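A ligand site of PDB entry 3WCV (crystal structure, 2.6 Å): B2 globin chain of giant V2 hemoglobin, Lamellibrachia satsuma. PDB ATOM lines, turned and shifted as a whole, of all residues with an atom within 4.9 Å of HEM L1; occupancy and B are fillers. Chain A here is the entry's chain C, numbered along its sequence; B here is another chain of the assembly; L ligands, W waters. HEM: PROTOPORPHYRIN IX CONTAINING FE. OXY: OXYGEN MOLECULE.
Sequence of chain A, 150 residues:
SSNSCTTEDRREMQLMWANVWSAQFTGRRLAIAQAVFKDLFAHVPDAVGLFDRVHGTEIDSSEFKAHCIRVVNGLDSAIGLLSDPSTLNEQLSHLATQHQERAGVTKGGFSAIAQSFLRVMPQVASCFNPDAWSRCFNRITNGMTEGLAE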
ATOM      1  N   LEU A  40     -29.638   1.260  33.707  1.00  0.00           N
ATOM      2  CA  LEU A  40     -28.263   1.695  33.485  1.00  0.00           C
ATOM      3  C   LEU A  40     -28.191   3.234  33.635  1.00  0.00           C
ATOM      4  O   LEU A  40     -27.343   3.769  34.350  1.00  0.00           O
ATOM      5  CB  LEU A  40     -27.655   1.282  32.090  1.00  0.00           C
ATOM      6  CG  LEU A  40     -26.313   1.837  31.804  1.00  0.00           C
ATOM      7  CD1 LEU A  40     -25.540   1.640  33.122  1.00  0.00           C
ATOM      8  CD2 LEU A  40     -25.671   0.925  30.762  1.00  0.00           C
ATOM      9  N   LEU A  50     -24.712   8.954  25.122  1.00  0.00           N
ATOM     10  CA  LEU A  50     -24.184   8.057  24.100  1.00  0.00           C
ATOM     11  C   LEU A  50     -25.263   7.564  23.157  1.00  0.00           C
ATOM     12  O   LEU A  50     -24.957   7.018  22.094  1.00  0.00           O
ATOM     13  CB  LEU A  50     -23.508   6.875  24.772  1.00  0.00           C
ATOM     14  CG  LEU A  50     -22.440   7.257  25.799  1.00  0.00           C
ATOM     15  CD1 LEU A  50     -22.085   6.065  26.660  1.00  0.00           C
ATOM     16  CD2 LEU A  50     -21.222   7.791  25.076  1.00  0.00           C
ATOM     17  N   PHE A  51     -26.525   7.763  23.529  1.00  0.00           N
ATOM     18  CA  PHE A  51     -27.647   7.280  22.716  1.00  0.00           C
ATOM     19  C   PHE A  51     -28.526   8.374  22.125  1.00  0.00           C
ATOM     20  O   PHE A  51     -29.719   8.158  21.863  1.00  0.00           O
ATOM     21  CB  PHE A  51     -28.491   6.328  23.567  1.00  0.00           C
ATOM     22  CG  PHE A  51     -27.699   5.203  24.179  1.00  0.00           C
ATOM     23  CD1 PHE A  51     -27.512   4.008  23.485  1.00  0.00           C
ATOM     24  CD2 PHE A  51     -27.067   5.378  25.414  1.00  0.00           C
ATOM     25  CE1 PHE A  51     -26.698   3.000  24.007  1.00  0.00           C
ATOM     26  CE2 PHE A  51     -26.255   4.373  25.950  1.00  0.00           C
ATOM     27  CZ  PHE A  51     -26.066   3.183  25.247  1.00  0.00           C
ATOM     28  N   ARG A  53     -28.527   9.560  19.146  1.00  0.00           N
ATOM     29  CA  ARG A  53     -28.983   9.230  17.802  1.00  0.00           C
ATOM     30  C   ARG A  53     -30.253   8.377  17.854  1.00  0.00           C
ATOM     31  O   ARG A  53     -31.090   8.440  16.954  1.00  0.00           O
ATOM     32  CB  ARG A  53     -27.895   8.477  17.029  1.00  0.00           C
ATOM     33  CG  ARG A  53     -28.216   8.323  15.549  1.00  0.00           C
ATOM     34  CD  ARG A  53     -27.283   7.333  14.894  1.00  0.00           C
ATOM     35  NE  ARG A  53     -27.714   5.960  15.121  1.00  0.00           N
ATOM     36  CZ  ARG A  53     -28.706   5.360  14.454  1.00  0.00           C
ATOM     37  NH1 ARG A  53     -29.026   4.102  14.718  1.00  0.00           N
ATOM     38  NH2 ARG A  53     -29.366   6.016  13.512  1.00  0.00           N
ATOM     39  N   VAL A  54     -30.385   7.583  18.911  1.00  0.00           N
ATOM     40  CA  VAL A  54     -31.538   6.706  19.092  1.00  0.00           C
ATOM     41  C   VAL A  54     -32.520   7.259  20.123  1.00  0.00           C
ATOM     42  O   VAL A  54     -33.406   6.534  20.603  1.00  0.00           O
ATOM     43  CB  VAL A  54     -31.073   5.288  19.532  1.00  0.00           C
ATOM     44  CG1 VAL A  54     -30.270   4.633  18.398  1.00  0.00           C
ATOM     45  CG2 VAL A  54     -30.225   5.369  20.790  1.00  0.00           C
ATOM     46  N   HIS A  67     -33.960   0.508  18.777  1.00  0.00           N
ATOM     47  CA  HIS A  67     -32.592   0.295  19.201  1.00  0.00           C
ATOM     48  C   HIS A  67     -32.542  -0.809  20.245  1.00  0.00           C
ATOM     49  O   HIS A  67     -31.662  -1.680  20.230  1.00  0.00           O
ATOM     50  CB  HIS A  67     -32.017   1.572  19.811  1.00  0.00           C
ATOM     51  CG  HIS A  67     -30.726   1.366  20.537  1.00  0.00           C
ATOM     52  ND1 HIS A  67     -29.563   0.999  19.892  1.00  0.00           N
ATOM     53  CD2 HIS A  67     -30.429   1.443  21.854  1.00  0.00           C
ATOM     54  CE1 HIS A  67     -28.596   0.866  20.787  1.00  0.00           C
ATOM     55  NE2 HIS A  67     -29.093   1.138  21.984  1.00  0.00           N
ATOM     56  N   ARG A  70     -32.791  -3.992  18.736  1.00  0.00           N
ATOM     57  CA  ARG A  70     -31.511  -4.365  18.113  1.00  0.00           C
ATOM     58  C   ARG A  70     -30.549  -4.877  19.163  1.00  0.00           C
ATOM     59  O   ARG A  70     -29.802  -5.825  18.915  1.00  0.00           O
ATOM     60  CB  ARG A  70     -30.880  -3.166  17.373  1.00  0.00           C
ATOM     61  CG  ARG A  70     -31.474  -2.891  15.987  1.00  0.00           C
ATOM     62  CD  ARG A  70     -30.605  -1.942  15.163  1.00  0.00           C
ATOM     63  NE  ARG A  70     -30.478  -0.609  15.784  1.00  0.00           N
ATOM     64  CZ  ARG A  70     -31.361   0.378  15.631  1.00  0.00           C
ATOM     65  NH1 ARG A  70     -32.444   0.193  14.894  1.00  0.00           N
ATOM     66  NH2 ARG A  70     -31.186   1.550  16.232  1.00  0.00           N
ATOM     67  N   VAL A  71     -30.535  -4.256  20.331  1.00  0.00           N
ATOM     68  CA  VAL A  71     -29.643  -4.726  21.381  1.00  0.00           C
ATOM     69  C   VAL A  71     -30.065  -6.151  21.770  1.00  0.00           C
ATOM     70  O   VAL A  71     -29.233  -7.066  21.838  1.00  0.00           O
ATOM     71  CB  VAL A  71     -29.691  -3.814  22.624  1.00  0.00           C
ATOM     72  CG1 VAL A  71     -28.745  -4.364  23.695  1.00  0.00           C
ATOM     73  CG2 VAL A  71     -29.312  -2.397  22.245  1.00  0.00           C
ATOM     74  N   GLY A  74     -29.097  -8.642  19.470  1.00  0.00           N
ATOM     75  CA  GLY A  74     -27.685  -8.933  19.530  1.00  0.00           C
ATOM     76  C   GLY A  74     -27.376  -9.923  20.630  1.00  0.00           C
ATOM     77  O   GLY A  74     -26.565 -10.828  20.434  1.00  0.00           O
ATOM     78  N   LEU A  75     -28.019  -9.736  21.777  1.00  0.00           N
ATOM     79  CA  LEU A  75     -27.835 -10.610  22.923  1.00  0.00           C
ATOM     80  C   LEU A  75     -28.408 -11.984  22.602  1.00  0.00           C
ATOM     81  O   LEU A  75     -27.815 -13.022  22.938  1.00  0.00           O
ATOM     82  CB  LEU A  75     -28.525 -10.012  24.142  1.00  0.00           C
ATOM     83  CG  LEU A  75     -28.156 -10.756  25.423  1.00  0.00           C
ATOM     84  CD1 LEU A  75     -26.630 -10.899  25.504  1.00  0.00           C
ATOM     85  CD2 LEU A  75     -28.742 -10.023  26.665  1.00  0.00           C
ATOM     86  N   LEU A  95     -19.610  -7.402  16.741  1.00  0.00           N
ATOM     87  CA  LEU A  95     -20.281  -6.540  17.709  1.00  0.00           C
ATOM     88  C   LEU A  95     -19.264  -5.599  18.321  1.00  0.00           C
ATOM     89  O   LEU A  95     -19.545  -4.426  18.584  1.00  0.00           O
ATOM     90  CB  LEU A  95     -20.964  -7.370  18.817  1.00  0.00           C
ATOM     91  CG  LEU A  95     -22.253  -8.117  18.450  1.00  0.00           C
ATOM     92  CD1 LEU A  95     -22.719  -8.913  19.662  1.00  0.00           C
ATOM     93  CD2 LEU A  95     -23.327  -7.127  18.004  1.00  0.00           C
ATOM     94  N   GLN A  98     -18.637  -2.773  16.362  1.00  0.00           N
ATOM     95  CA  GLN A  98     -19.823  -1.915  16.326  1.00  0.00           C
ATOM     96  C   GLN A  98     -19.871  -1.012  17.563  1.00  0.00           C
ATOM     97  O   GLN A  98     -20.580  -0.004  17.568  1.00  0.00           O
ATOM     98  CB  GLN A  98     -21.106  -2.756  16.225  1.00  0.00           C
ATOM     99  CG  GLN A  98     -21.353  -3.376  14.839  1.00  0.00           C
ATOM    100  CD  GLN A  98     -22.684  -4.101  14.754  1.00  0.00           C
ATOM    101  OE1 GLN A  98     -23.016  -4.903  15.630  1.00  0.00           O
ATOM    102  NE2 GLN A  98     -23.443  -3.854  13.700  1.00  0.00           N
ATOM    103  N   HIS A  99     -19.113  -1.364  18.598  1.00  0.00           N
ATOM    104  CA  HIS A  99     -19.063  -0.580  19.830  1.00  0.00           C
ATOM    105  C   HIS A  99     -17.732   0.118  19.958  1.00  0.00           C
ATOM    106  O   HIS A  99     -17.562   1.064  20.752  1.00  0.00           O
ATOM    107  CB  HIS A  99     -19.289  -1.485  21.036  1.00  0.00           C
ATOM    108  CG  HIS A  99     -20.698  -1.976  21.155  1.00  0.00           C
ATOM    109  ND1 HIS A  99     -21.246  -2.880  20.270  1.00  0.00           N
ATOM    110  CD2 HIS A  99     -21.689  -1.648  22.016  1.00  0.00           C
ATOM    111  CE1 HIS A  99     -22.516  -3.085  20.589  1.00  0.00           C
ATOM    112  NE2 HIS A  99     -22.803  -2.346  21.646  1.00  0.00           N
ATOM    113  N   ARG A 102     -16.242   4.703  19.747  1.00  0.00           N
ATOM    114  CA  ARG A 102     -17.455   5.399  20.083  1.00  0.00           C
ATOM    115  C   ARG A 102     -17.129   5.830  21.498  1.00  0.00           C
ATOM    116  O   ARG A 102     -17.248   5.052  22.436  1.00  0.00           O
ATOM    117  CB  ARG A 102     -18.639   4.482  20.040  1.00  0.00           C
ATOM    118  CG  ARG A 102     -19.482   4.670  18.822  1.00  0.00           C
ATOM    119  CD  ARG A 102     -20.869   4.147  19.034  1.00  0.00           C
ATOM    120  NE  ARG A 102     -21.108   2.930  18.270  1.00  0.00           N
ATOM    121  CZ  ARG A 102     -21.890   2.841  17.202  1.00  0.00           C
ATOM    122  NH1 ARG A 102     -22.030   1.684  16.582  1.00  0.00           N
ATOM    123  NH2 ARG A 102     -22.542   3.919  16.758  1.00  0.00           N
ATOM    124  N   VAL A 105     -18.182   4.524  25.235  1.00  0.00           N
ATOM    125  CA  VAL A 105     -18.470   3.090  25.177  1.00  0.00           C
ATOM    126  C   VAL A 105     -17.115   2.619  25.712  1.00  0.00           C
ATOM    127  O   VAL A 105     -16.102   2.843  25.085  1.00  0.00           O
ATOM    128  CB  VAL A 105     -18.685   2.590  23.754  1.00  0.00           C
ATOM    129  CG1 VAL A 105     -19.009   1.131  23.769  1.00  0.00           C
ATOM    130  CG2 VAL A 105     -19.701   3.415  23.011  1.00  0.00           C
ATOM    131  N   GLY A 109     -18.814   0.695  31.228  1.00  0.00           N
ATOM    132  CA  GLY A 109     -20.235   0.726  30.941  1.00  0.00           C
ATOM    133  C   GLY A 109     -20.839  -0.659  30.786  1.00  0.00           C
ATOM    134  O   GLY A 109     -22.022  -0.871  31.070  1.00  0.00           O
ATOM    135  N   PHE A 110     -20.022  -1.602  30.328  1.00  0.00           N
ATOM    136  CA  PHE A 110     -20.476  -2.964  30.135  1.00  0.00           C
ATOM    137  C   PHE A 110     -20.645  -3.641  31.475  1.00  0.00           C
ATOM    138  O   PHE A 110     -21.571  -4.435  31.662  1.00  0.00           O
ATOM    139  CB  PHE A 110     -19.488  -3.720  29.242  1.00  0.00           C
ATOM    140  CG  PHE A 110     -19.809  -3.610  27.774  1.00  0.00           C
ATOM    141  CD1 PHE A 110     -20.520  -4.620  27.136  1.00  0.00           C
ATOM    142  CD2 PHE A 110     -19.428  -2.483  27.043  1.00  0.00           C
ATOM    143  CE1 PHE A 110     -20.854  -4.527  25.787  1.00  0.00           C
ATOM    144  CE2 PHE A 110     -19.759  -2.370  25.683  1.00  0.00           C
ATOM    145  CZ  PHE A 110     -20.464  -3.391  25.063  1.00  0.00           C
ATOM    146  N   ILE A 113     -24.026  -2.216  32.746  1.00  0.00           N
ATOM    147  CA  ILE A 113     -25.180  -2.883  32.170  1.00  0.00           C
ATOM    148  C   ILE A 113     -25.280  -4.337  32.622  1.00  0.00           C
ATOM    149  O   ILE A 113     -26.382  -4.888  32.721  1.00  0.00           O
ATOM    150  CB  ILE A 113     -25.153  -2.798  30.629  1.00  0.00           C
ATOM    151  CG1 ILE A 113     -26.577  -2.892  30.105  1.00  0.00           C
ATOM    152  CG2 ILE A 113     -24.290  -3.918  30.043  1.00  0.00           C
ATOM    153  CD1 ILE A 113     -26.707  -2.564  28.648  1.00  0.00           C
ATOM    154  N   PHE A 137     -22.713 -14.147  30.620  1.00  0.00           N
ATOM    155  CA  PHE A 137     -22.948 -12.810  30.129  1.00  0.00           C
ATOM    156  C   PHE A 137     -21.556 -12.220  29.962  1.00  0.00           C
ATOM    157  O   PHE A 137     -21.234 -11.657  28.920  1.00  0.00           O
ATOM    158  CB  PHE A 137     -23.734 -11.984  31.159  1.00  0.00           C
ATOM    159  CG  PHE A 137     -24.190 -10.653  30.653  1.00  0.00           C
ATOM    160  CD1 PHE A 137     -25.315 -10.542  29.831  1.00  0.00           C
ATOM    161  CD2 PHE A 137     -23.489  -9.497  30.997  1.00  0.00           C
ATOM    162  CE1 PHE A 137     -25.739  -9.287  29.356  1.00  0.00           C
ATOM    163  CE2 PHE A 137     -23.904  -8.243  30.524  1.00  0.00           C
ATOM    164  CZ  PHE A 137     -25.028  -8.140  29.697  1.00  0.00           C
ATOM    165  N   ILE A 140     -19.659 -13.319  27.121  1.00  0.00           N
ATOM    166  CA  ILE A 140     -20.162 -12.618  25.952  1.00  0.00           C
ATOM    167  C   ILE A 140     -19.628 -11.200  25.836  1.00  0.00           C
ATOM    168  O   ILE A 140     -19.195 -10.786  24.759  1.00  0.00           O
ATOM    169  CB  ILE A 140     -21.709 -12.608  25.950  1.00  0.00           C
ATOM    170  CG1 ILE A 140     -22.213 -13.977  25.478  1.00  0.00           C
ATOM    171  CG2 ILE A 140     -22.267 -11.454  25.070  1.00  0.00           C
ATOM    172  CD1 ILE A 140     -23.703 -14.148  25.565  1.00  0.00           C
ATOM    173  N   THR A 141     -19.649 -10.451  26.945  1.00  0.00           N
ATOM    174  CA  THR A 141     -19.141  -9.080  26.901  1.00  0.00           C
ATOM    175  C   THR A 141     -17.630  -9.065  26.611  1.00  0.00           C
ATOM    176  O   THR A 141     -17.167  -8.251  25.807  1.00  0.00           O
ATOM    177  CB  THR A 141     -19.434  -8.296  28.227  1.00  0.00           C
ATOM    178  OG1 THR A 141     -18.806  -8.940  29.338  1.00  0.00           O
ATOM    179  CG2 THR A 141     -20.940  -8.185  28.466  1.00  0.00           C
ATOM    180  N   MET A 144     -17.084  -8.784  23.271  1.00  0.00           N
ATOM    181  CA  MET A 144     -17.583  -7.524  22.759  1.00  0.00           C
ATOM    182  C   MET A 144     -16.690  -6.319  23.067  1.00  0.00           C
ATOM    183  O   MET A 144     -16.669  -5.346  22.316  1.00  0.00           O
ATOM    184  CB  MET A 144     -18.980  -7.241  23.324  1.00  0.00           C
ATOM    185  CG  MET A 144     -20.066  -8.177  22.809  1.00  0.00           C
ATOM    186  SD  MET A 144     -21.679  -7.689  23.493  1.00  0.00           S
ATOM    187  CE  MET A 144     -22.181  -6.467  22.282  1.00  0.00           C
ATOM    188  N   HIS B  90     -33.276   1.332   9.214  1.00  0.00           N
ATOM    189  CA  HIS B  90     -31.942   0.998   9.734  1.00  0.00           C
ATOM    190  C   HIS B  90     -31.283  -0.001   8.797  1.00  0.00           C
ATOM    191  O   HIS B  90     -30.094   0.126   8.460  1.00  0.00           O
ATOM    192  CB  HIS B  90     -32.026   0.390  11.124  1.00  0.00           C
ATOM    193  CG  HIS B  90     -30.702   0.234  11.792  1.00  0.00           C
ATOM    194  ND1 HIS B  90     -30.054   1.294  12.400  1.00  0.00           N
ATOM    195  CD2 HIS B  90     -29.894  -0.833  11.951  1.00  0.00           C
ATOM    196  CE1 HIS B  90     -28.906   0.871  12.909  1.00  0.00           C
ATOM    197  NE2 HIS B  90     -28.783  -0.419  12.646  1.00  0.00           N
ATOM    198  N   GLN B  94     -27.907   0.144   6.246  1.00  0.00           N
ATOM    199  CA  GLN B  94     -26.817  -0.825   6.335  1.00  0.00           C
ATOM    200  C   GLN B  94     -26.518  -1.430   4.968  1.00  0.00           C
ATOM    201  O   GLN B  94     -25.463  -2.034   4.788  1.00  0.00           O
ATOM    202  CB  GLN B  94     -27.179  -1.936   7.346  1.00  0.00           C
ATOM    203  CG  GLN B  94     -27.345  -1.441   8.792  1.00  0.00           C
ATOM    204  CD  GLN B  94     -27.722  -2.550   9.777  1.00  0.00           C
ATOM    205  OE1 GLN B  94     -28.739  -3.242   9.599  1.00  0.00           O
ATOM    206  NE2 GLN B  94     -26.916  -2.724  10.815  1.00  0.00           N
HETATM  207  CHA HEM L   1     -25.356  -0.230  19.369  1.00  0.00           C
HETATM  208  CHB HEM L   1     -25.804  -4.560  21.207  1.00  0.00           C
HETATM  209  CHC HEM L   1     -23.986  -3.022  25.417  1.00  0.00           C
HETATM  210  CHD HEM L   1     -23.488   1.356  23.487  1.00  0.00           C
HETATM  211  C1A HEM L   1     -25.641  -1.547  19.483  1.00  0.00           C
HETATM  212  C2A HEM L   1     -26.203  -2.304  18.435  1.00  0.00           C
HETATM  213  C3A HEM L   1     -26.325  -3.553  18.952  1.00  0.00           C
HETATM  214  C4A HEM L   1     -25.840  -3.550  20.335  1.00  0.00           C
HETATM  215  CMA HEM L   1     -26.891  -4.794  18.247  1.00  0.00           C
HETATM  216  CAA HEM L   1     -26.590  -1.826  17.030  1.00  0.00           C
HETATM  217  CBA HEM L   1     -25.529  -2.056  15.981  1.00  0.00           C
HETATM  218  CGA HEM L   1     -25.892  -1.585  14.552  1.00  0.00           C
HETATM  219  O1A HEM L   1     -26.894  -2.088  13.957  1.00  0.00           O
HETATM  220  O2A HEM L   1     -25.209  -0.748  14.039  1.00  0.00           O
HETATM  221  C1B HEM L   1     -25.352  -4.557  22.546  1.00  0.00           C
HETATM  222  C2B HEM L   1     -25.376  -5.727  23.424  1.00  0.00           C
HETATM  223  C3B HEM L   1     -24.836  -5.255  24.683  1.00  0.00           C
HETATM  224  C4B HEM L   1     -24.528  -3.870  24.461  1.00  0.00           C
HETATM  225  CMB HEM L   1     -25.862  -7.082  23.084  1.00  0.00           C
HETATM  226  CAB HEM L   1     -24.676  -6.091  25.860  1.00  0.00           C
HETATM  227  CBB HEM L   1     -23.667  -6.905  26.090  1.00  0.00           C
HETATM  228  C1C HEM L   1     -23.687  -1.685  25.234  1.00  0.00           C
HETATM  229  C2C HEM L   1     -23.097  -0.851  26.313  1.00  0.00           C
HETATM  230  C3C HEM L   1     -22.928   0.448  25.777  1.00  0.00           C
HETATM  231  C4C HEM L   1     -23.454   0.311  24.360  1.00  0.00           C
HETATM  232  CMC HEM L   1     -22.732  -1.325  27.728  1.00  0.00           C
HETATM  233  CAC HEM L   1     -22.413   1.551  26.395  1.00  0.00           C
HETATM  234  CBC HEM L   1     -22.546   2.233  27.486  1.00  0.00           C
HETATM  235  C1D HEM L   1     -23.968   1.310  22.175  1.00  0.00           C
HETATM  236  C2D HEM L   1     -24.005   2.518  21.249  1.00  0.00           C
HETATM  237  C3D HEM L   1     -24.555   2.027  20.096  1.00  0.00           C
HETATM  238  C4D HEM L   1     -24.812   0.592  20.309  1.00  0.00           C
HETATM  239  CMD HEM L   1     -23.540   3.909  21.606  1.00  0.00           C
HETATM  240  CAD HEM L   1     -24.851   2.779  18.811  1.00  0.00           C
HETATM  241  CBD HEM L   1     -26.322   3.155  18.817  1.00  0.00           C
HETATM  242  CGD HEM L   1     -26.790   3.870  17.629  1.00  0.00           C
HETATM  243  O1D HEM L   1     -26.725   5.126  17.586  1.00  0.00           O
HETATM  244  O2D HEM L   1     -27.264   3.221  16.682  1.00  0.00           O
HETATM  245  NA  HEM L   1     -25.404  -2.290  20.651  1.00  0.00           N
HETATM  246  NB  HEM L   1     -24.862  -3.451  23.138  1.00  0.00           N
HETATM  247  NC  HEM L   1     -23.877  -0.941  24.088  1.00  0.00           N
HETATM  248  ND  HEM L   1     -24.454   0.215  21.567  1.00  0.00           N
HETATM  249 FE   HEM L   1     -24.634  -1.622  22.361  1.00  0.00          FE
HETATM  250  O1  OXY L   2     -26.188  -0.986  22.984  1.00  0.00           O
HETATM  251  O2  OXY L   2     -27.036  -0.113  23.210  1.00  0.00           O
HETATM  252  O   HOH W   1     -29.216   0.798  17.383  1.00  0.00           O
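An iron atom (FE) of HEM L1 is bound by a ring nitrogen (NE2) of His 99. The guanidinium group (NH1) of Arg 53 is in salt-bridge range of an oxygen (O2D) of HEM L1. An oxygen (O1A) of HEM L1 sits at hydrogen-bond distance from a ring nitrogen (NE2) of His 90 of chain B, at 2.8 Å. The side-chain amide nitrogen of Gln 94 of chain B is in hydrogen-bond range of an oxygen (O1A) of HEM L1 (3.2 Å). O2 of OXY L2 is in hydrogen-bond range of NE2 of His 67 (2.7 Å).
O1 of OXY L2 is bound to FE of HEM L1 (1.8 Å).
A ring nitrogen (ND1) of His 99 lies within hydrogen-bond range of the backbone carbonyl oxygen (O) of Leu 95 (2.9 Å). A ring nitrogen (NE2) of His 90 of chain B sits at hydrogen-bond distance from the side-chain amide nitrogen (NE2) of Gln 94 of chain B, at 3.5 Å. NH1 of Arg 102 lies within hydrogen-bond range of O of Gln 98, at 2.4 Å.
Merely in contact with HEM L1: Arg 70, Arg 102, Met 144, Gln 98, Gly 109, Leu 50, Phe 110, Val 71, Phe 51, Val 54, Leu 75, His 67, Ile 113 and Thr 141. Hydrophobic or aromatic side chains within 4 Å of HEM L1: Leu 50, Phe 51, Val 54, His 67, Val 71, His 99, Phe 110, Ile 113, Met 144 and His 90 of chain B. 18 residues have an atom within 4 Å of HEM L1: Leu 50, Phe 51, Arg 53, Val 54, His 67, Arg 70, Val 71, Leu 75, Gln 98, His 99, Arg 102, Gly 109, Phe 110, Ile 113, Thr 141, Met 144, His 90 of chain B and Gln 94 of chain B. The nearest printed residue that does not touch HEM L1 is Gly 74 (4.05 Å).
Water W1 lies within hydrogen-bond range of NH2 of Arg 70, ND1 of His 67 and O2D of HEM L1.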
